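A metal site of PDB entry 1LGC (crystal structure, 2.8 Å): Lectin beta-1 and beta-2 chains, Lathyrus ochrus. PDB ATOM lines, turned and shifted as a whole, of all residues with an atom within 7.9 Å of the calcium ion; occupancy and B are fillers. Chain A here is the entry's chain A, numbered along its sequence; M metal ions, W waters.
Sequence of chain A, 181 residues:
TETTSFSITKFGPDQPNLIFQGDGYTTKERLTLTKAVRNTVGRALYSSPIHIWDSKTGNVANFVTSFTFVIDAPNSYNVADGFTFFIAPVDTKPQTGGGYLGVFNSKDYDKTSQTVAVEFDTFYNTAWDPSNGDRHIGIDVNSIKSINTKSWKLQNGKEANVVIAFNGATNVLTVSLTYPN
OD1 of Asp 129 sits close to NE2 of His 136 (3.0 Å).
The backbone NH (N) of Thr 122 is in hydrogen-bond range of the backbone carbonyl oxygen (O) of Asp 81 (2.8 Å).
The backbone NH (N) of Asn 125 lies within hydrogen-bond range of the side-chain carboxylate (OD2) of Asp 129.
The backbone NH (N) of Asp 121 sits at hydrogen-bond distance from the backbone carbonyl oxygen (O) of His 136 (2.9 Å).
OD1 of Asn 125 binds the calcium ion, at 2.0 Å.
The backbone carbonyl oxygen (O) of Phe 123 is bound to the calcium ion, at 2.0 Å.
Water W1 binds the calcium ion, at 2.1 Å.
OD1 of Asp 121 binds the calcium ion (2.3 Å).
The calcium ion is bound by OD2 of Asp 121, 2.5 Å away.
OD1 of Asp 81 is bound to the calcium ion.
The calcium ion has six donor atoms within binding distance.
Slightly farther from the calcium ion lies OD2 of Asp 129 (3.1 Å).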
ATOM      1  N   VAL A  79      -7.073 -24.011  10.991  1.00  0.00           N
ATOM      2  CA  VAL A  79      -7.917 -23.468  12.036  1.00  0.00           C
ATOM      3  C   VAL A  79      -8.015 -21.968  11.904  1.00  0.00           C
ATOM      4  O   VAL A  79      -7.050 -21.304  11.551  1.00  0.00           O
ATOM      5  CB  VAL A  79      -7.324 -23.779  13.406  1.00  0.00           C
ATOM      6  CG1 VAL A  79      -8.183 -23.158  14.515  1.00  0.00           C
ATOM      7  CG2 VAL A  79      -7.187 -25.289  13.596  1.00  0.00           C
ATOM      8  N   ALA A  80      -9.194 -21.424  12.187  1.00  0.00           N
ATOM      9  CA  ALA A  80      -9.407 -19.991  12.111  1.00  0.00           C
ATOM     10  C   ALA A  80     -10.780 -19.612  12.672  1.00  0.00           C
ATOM     11  O   ALA A  80     -11.723 -20.396  12.598  1.00  0.00           O
ATOM     12  CB  ALA A  80      -9.278 -19.520  10.670  1.00  0.00           C
ATOM     13  N   ASP A  81     -10.902 -18.408  13.216  1.00  0.00           N
ATOM     14  CA  ASP A  81      -9.773 -17.503  13.282  1.00  0.00           C
ATOM     15  C   ASP A  81      -9.349 -17.242  14.712  1.00  0.00           C
ATOM     16  O   ASP A  81      -8.152 -17.182  14.995  1.00  0.00           O
ATOM     17  CB  ASP A  81     -10.044 -16.186  12.585  1.00  0.00           C
ATOM     18  CG  ASP A  81      -8.792 -15.351  12.465  1.00  0.00           C
ATOM     19  OD1 ASP A  81      -8.283 -14.857  13.502  1.00  0.00           O
ATOM     20  OD2 ASP A  81      -8.290 -15.240  11.334  1.00  0.00           O
ATOM     21  N   GLY A  82     -10.304 -17.023  15.613  1.00  0.00           N
ATOM     22  CA  GLY A  82      -9.961 -16.776  16.991  1.00  0.00           C
ATOM     23  C   GLY A  82     -11.125 -16.448  17.911  1.00  0.00           C
ATOM     24  O   GLY A  82     -12.225 -16.083  17.506  1.00  0.00           O
ATOM     25  N   GLY A  98     -14.035 -12.390  10.229  1.00  0.00           N
ATOM     26  CA  GLY A  98     -12.791 -12.973   9.744  1.00  0.00           C
ATOM     27  C   GLY A  98     -11.601 -12.783  10.668  1.00  0.00           C
ATOM     28  O   GLY A  98     -11.722 -12.902  11.880  1.00  0.00           O
ATOM     29  N   GLY A  99     -10.462 -12.434  10.090  1.00  0.00           N
ATOM     30  CA  GLY A  99      -9.264 -12.248  10.880  1.00  0.00           C
ATOM     31  C   GLY A  99      -9.335 -11.112  11.890  1.00  0.00           C
ATOM     32  O   GLY A  99      -8.476 -11.065  12.786  1.00  0.00           O
ATOM     33  N   TYR A 100     -10.316 -10.219  11.734  1.00  0.00           N
ATOM     34  CA  TYR A 100     -10.495  -9.066  12.631  1.00  0.00           C
ATOM     35  C   TYR A 100     -11.309  -9.407  13.876  1.00  0.00           C
ATOM     36  O   TYR A 100     -11.820  -8.514  14.564  1.00  0.00           O
ATOM     37  CB  TYR A 100     -11.170  -7.905  11.908  1.00  0.00           C
ATOM     38  CG  TYR A 100     -10.256  -7.125  10.994  1.00  0.00           C
ATOM     39  CD1 TYR A 100      -9.439  -6.126  11.502  1.00  0.00           C
ATOM     40  CD2 TYR A 100     -10.253  -7.356   9.621  1.00  0.00           C
ATOM     41  CE1 TYR A 100      -8.625  -5.386  10.672  1.00  0.00           C
ATOM     42  CE2 TYR A 100      -9.449  -6.617   8.789  1.00  0.00           C
ATOM     43  CZ  TYR A 100      -8.645  -5.632   9.312  1.00  0.00           C
ATOM     44  OH  TYR A 100      -7.849  -4.871   8.473  1.00  0.00           O
ATOM     45  N   LEU A 101     -11.488 -10.704  14.104  1.00  0.00           N
ATOM     46  CA  LEU A 101     -12.190 -11.228  15.263  1.00  0.00           C
ATOM     47  C   LEU A 101     -13.554 -10.629  15.642  1.00  0.00           C
ATOM     48  O   LEU A 101     -14.115 -10.978  16.670  1.00  0.00           O
ATOM     49  CB  LEU A 101     -11.247 -11.248  16.477  1.00  0.00           C
ATOM     50  CG  LEU A 101      -9.987 -12.086  16.204  1.00  0.00           C
ATOM     51  CD1 LEU A 101      -9.074 -12.055  17.411  1.00  0.00           C
ATOM     52  CD2 LEU A 101     -10.378 -13.505  15.859  1.00  0.00           C
ATOM     53  N   GLU A 119      -7.222 -11.465  23.029  1.00  0.00           N
ATOM     54  CA  GLU A 119      -7.476 -12.410  21.955  1.00  0.00           C
ATOM     55  C   GLU A 119      -6.671 -13.696  21.992  1.00  0.00           C
ATOM     56  O   GLU A 119      -5.511 -13.712  22.398  1.00  0.00           O
ATOM     57  CB  GLU A 119      -7.184 -11.737  20.612  1.00  0.00           C
ATOM     58  CG  GLU A 119      -5.750 -11.232  20.506  1.00  0.00           C
ATOM     59  CD  GLU A 119      -5.267 -11.067  19.090  1.00  0.00           C
ATOM     60  OE1 GLU A 119      -5.833 -10.243  18.342  1.00  0.00           O
ATOM     61  OE2 GLU A 119      -4.314 -11.766  18.716  1.00  0.00           O
ATOM     62  N   PHE A 120      -7.274 -14.757  21.487  1.00  0.00           N
ATOM     63  CA  PHE A 120      -6.659 -16.059  21.406  1.00  0.00           C
ATOM     64  C   PHE A 120      -6.854 -16.276  19.910  1.00  0.00           C
ATOM     65  O   PHE A 120      -7.952 -16.595  19.459  1.00  0.00           O
ATOM     66  CB  PHE A 120      -7.457 -17.048  22.261  1.00  0.00           C
ATOM     67  CG  PHE A 120      -7.567 -16.638  23.741  1.00  0.00           C
ATOM     68  CD1 PHE A 120      -8.597 -15.823  24.185  1.00  0.00           C
ATOM     69  CD2 PHE A 120      -6.611 -17.060  24.666  1.00  0.00           C
ATOM     70  CE1 PHE A 120      -8.674 -15.422  25.513  1.00  0.00           C
ATOM     71  CE2 PHE A 120      -6.690 -16.652  26.006  1.00  0.00           C
ATOM     72  CZ  PHE A 120      -7.714 -15.841  26.419  1.00  0.00           C
ATOM     73  N   ASP A 121      -5.799 -15.948  19.153  1.00  0.00           N
ATOM     74  CA  ASP A 121      -5.784 -16.007  17.683  1.00  0.00           C
ATOM     75  C   ASP A 121      -5.147 -17.266  17.125  1.00  0.00           C
ATOM     76  O   ASP A 121      -3.930 -17.435  17.178  1.00  0.00           O
ATOM     77  CB  ASP A 121      -5.046 -14.777  17.146  1.00  0.00           C
ATOM     78  CG  ASP A 121      -5.200 -14.572  15.641  1.00  0.00           C
ATOM     79  OD1 ASP A 121      -5.749 -15.449  14.935  1.00  0.00           O
ATOM     80  OD2 ASP A 121      -4.768 -13.508  15.149  1.00  0.00           O
ATOM     81  N   THR A 122      -5.974 -18.063  16.468  1.00  0.00           N
ATOM     82  CA  THR A 122      -5.546 -19.327  15.885  1.00  0.00           C
ATOM     83  C   THR A 122      -5.258 -19.286  14.380  1.00  0.00           C
ATOM     84  O   THR A 122      -5.207 -20.321  13.741  1.00  0.00           O
ATOM     85  CB  THR A 122      -6.603 -20.385  16.148  1.00  0.00           C
ATOM     86  OG1 THR A 122      -7.870 -19.899  15.710  1.00  0.00           O
ATOM     87  CG2 THR A 122      -6.680 -20.667  17.628  1.00  0.00           C
ATOM     88  N   PHE A 123      -5.028 -18.097  13.828  1.00  0.00           N
ATOM     89  CA  PHE A 123      -4.748 -17.969  12.402  1.00  0.00           C
ATOM     90  C   PHE A 123      -3.783 -16.823  12.138  1.00  0.00           C
ATOM     91  O   PHE A 123      -4.030 -15.670  12.550  1.00  0.00           O
ATOM     92  CB  PHE A 123      -6.050 -17.783  11.614  1.00  0.00           C
ATOM     93  CG  PHE A 123      -5.877 -17.820  10.120  1.00  0.00           C
ATOM     94  CD1 PHE A 123      -5.273 -16.763   9.446  1.00  0.00           C
ATOM     95  CD2 PHE A 123      -6.367 -18.891   9.376  1.00  0.00           C
ATOM     96  CE1 PHE A 123      -5.146 -16.785   8.070  1.00  0.00           C
ATOM     97  CE2 PHE A 123      -6.238 -18.910   7.991  1.00  0.00           C
ATOM     98  CZ  PHE A 123      -5.619 -17.848   7.342  1.00  0.00           C
ATOM     99  N   TYR A 124      -2.706 -17.136  11.431  1.00  0.00           N
ATOM    100  CA  TYR A 124      -1.676 -16.170  11.060  1.00  0.00           C
ATOM    101  C   TYR A 124      -2.151 -15.260   9.943  1.00  0.00           C
ATOM    102  O   TYR A 124      -2.465 -15.714   8.853  1.00  0.00           O
ATOM    103  CB  TYR A 124      -0.407 -16.910  10.601  1.00  0.00           C
ATOM    104  CG  TYR A 124       0.736 -15.990  10.182  1.00  0.00           C
ATOM    105  CD1 TYR A 124       1.064 -14.854  10.915  1.00  0.00           C
ATOM    106  CD2 TYR A 124       1.471 -16.261   9.024  1.00  0.00           C
ATOM    107  CE1 TYR A 124       2.070 -13.996  10.516  1.00  0.00           C
ATOM    108  CE2 TYR A 124       2.489 -15.411   8.616  1.00  0.00           C
ATOM    109  CZ  TYR A 124       2.784 -14.279   9.361  1.00  0.00           C
ATOM    110  OH  TYR A 124       3.756 -13.415   8.926  1.00  0.00           O
ATOM    111  N   ASN A 125      -2.219 -13.963  10.236  1.00  0.00           N
ATOM    112  CA  ASN A 125      -2.627 -12.980   9.232  1.00  0.00           C
ATOM    113  C   ASN A 125      -1.357 -12.202   8.937  1.00  0.00           C
ATOM    114  O   ASN A 125      -0.984 -11.314   9.701  1.00  0.00           O
ATOM    115  CB  ASN A 125      -3.681 -12.044   9.779  1.00  0.00           C
ATOM    116  CG  ASN A 125      -4.928 -12.765  10.204  1.00  0.00           C
ATOM    117  OD1 ASN A 125      -4.957 -13.385  11.282  1.00  0.00           O
ATOM    118  ND2 ASN A 125      -5.968 -12.694   9.387  1.00  0.00           N
ATOM    119  N   THR A 126      -0.723 -12.526   7.819  1.00  0.00           N
ATOM    120  CA  THR A 126       0.525 -11.895   7.437  1.00  0.00           C
ATOM    121  C   THR A 126       0.532 -10.352   7.526  1.00  0.00           C
ATOM    122  O   THR A 126       1.562  -9.729   7.815  1.00  0.00           O
ATOM    123  CB  THR A 126       1.006 -12.365   6.037  1.00  0.00           C
ATOM    124  OG1 THR A 126       0.151 -11.819   5.023  1.00  0.00           O
ATOM    125  CG2 THR A 126       0.977 -13.881   5.960  1.00  0.00           C
ATOM    126  N   TRP A 128      -0.669  -8.403   9.855  1.00  0.00           N
ATOM    127  CA  TRP A 128      -0.480  -7.808  11.187  1.00  0.00           C
ATOM    128  C   TRP A 128      -0.088  -8.732  12.357  1.00  0.00           C
ATOM    129  O   TRP A 128       0.203  -8.229  13.452  1.00  0.00           O
ATOM    130  CB  TRP A 128      -1.745  -7.044  11.580  1.00  0.00           C
ATOM    131  CG  TRP A 128      -2.931  -7.944  11.680  1.00  0.00           C
ATOM    132  CD1 TRP A 128      -3.153  -8.902  12.615  1.00  0.00           C
ATOM    133  CD2 TRP A 128      -4.057  -7.995  10.788  1.00  0.00           C
ATOM    134  NE1 TRP A 128      -4.347  -9.541  12.370  1.00  0.00           N
ATOM    135  CE2 TRP A 128      -4.922  -9.001  11.249  1.00  0.00           C
ATOM    136  CE3 TRP A 128      -4.421  -7.286   9.632  1.00  0.00           C
ATOM    137  CZ2 TRP A 128      -6.124  -9.321  10.619  1.00  0.00           C
ATOM    138  CZ3 TRP A 128      -5.623  -7.596   9.004  1.00  0.00           C
ATOM    139  CH2 TRP A 128      -6.454  -8.606   9.493  1.00  0.00           C
ATOM    140  N   ASP A 129      -0.146 -10.044  12.169  1.00  0.00           N
ATOM    141  CA  ASP A 129       0.215 -10.972  13.248  1.00  0.00           C
ATOM    142  C   ASP A 129       1.727 -11.182  13.315  1.00  0.00           C
ATOM    143  O   ASP A 129       2.428 -11.013  12.302  1.00  0.00           O
ATOM    144  CB  ASP A 129      -0.499 -12.306  13.069  1.00  0.00           C
ATOM    145  CG  ASP A 129      -1.917 -12.292  13.608  1.00  0.00           C
ATOM    146  OD1 ASP A 129      -2.108 -11.832  14.757  1.00  0.00           O
ATOM    147  OD2 ASP A 129      -2.844 -12.756  12.894  1.00  0.00           O
ATOM    148  N   ASP A 134       2.822 -18.205  14.911  1.00  0.00           N
ATOM    149  CA  ASP A 134       2.271 -19.126  15.896  1.00  0.00           C
ATOM    150  C   ASP A 134       0.907 -18.688  16.419  1.00  0.00           C
ATOM    151  O   ASP A 134       0.595 -17.501  16.428  1.00  0.00           O
ATOM    152  CB  ASP A 134       3.209 -19.254  17.087  1.00  0.00           C
ATOM    153  CG  ASP A 134       4.653 -19.423  16.667  1.00  0.00           C
ATOM    154  OD1 ASP A 134       4.910 -20.087  15.637  1.00  0.00           O
ATOM    155  OD2 ASP A 134       5.518 -18.880  17.384  1.00  0.00           O
ATOM    156  N   HIS A 136      -1.499 -17.551  19.124  1.00  0.00           N
ATOM    157  CA  HIS A 136      -1.065 -16.765  20.267  1.00  0.00           C
ATOM    158  C   HIS A 136      -2.158 -16.060  20.998  1.00  0.00           C
ATOM    159  O   HIS A 136      -3.214 -15.795  20.436  1.00  0.00           O
ATOM    160  CB  HIS A 136      -0.089 -15.715  19.766  1.00  0.00           C
ATOM    161  CG  HIS A 136      -0.621 -14.895  18.628  1.00  0.00           C
ATOM    162  ND1 HIS A 136      -0.666 -15.361  17.344  1.00  0.00           N
ATOM    163  CD2 HIS A 136      -1.139 -13.647  18.594  1.00  0.00           C
ATOM    164  CE1 HIS A 136      -1.182 -14.445  16.553  1.00  0.00           C
ATOM    165  NE2 HIS A 136      -1.477 -13.386  17.279  1.00  0.00           N
ATOM    166  N   ILE A 144      -6.423  -4.350  15.758  1.00  0.00           N
ATOM    167  CA  ILE A 144      -6.261  -5.799  15.695  1.00  0.00           C
ATOM    168  C   ILE A 144      -4.805  -6.267  15.874  1.00  0.00           C
ATOM    169  O   ILE A 144      -4.537  -7.457  16.023  1.00  0.00           O
ATOM    170  CB  ILE A 144      -6.895  -6.358  14.388  1.00  0.00           C
ATOM    171  CG1 ILE A 144      -7.621  -7.684  14.636  1.00  0.00           C
ATOM    172  CG2 ILE A 144      -5.871  -6.428  13.260  1.00  0.00           C
ATOM    173  CD1 ILE A 144      -6.741  -8.874  14.981  1.00  0.00           C
HETATM  174 CA    CA M   1      -5.511 -14.347  12.895  1.00  0.00          CA
HETATM  175 MN    MN M   2      -3.722 -11.318  16.609  1.00  0.00          MN
HETATM  176  O   HOH W   1      -6.368 -12.498  13.463  1.00  0.00           O
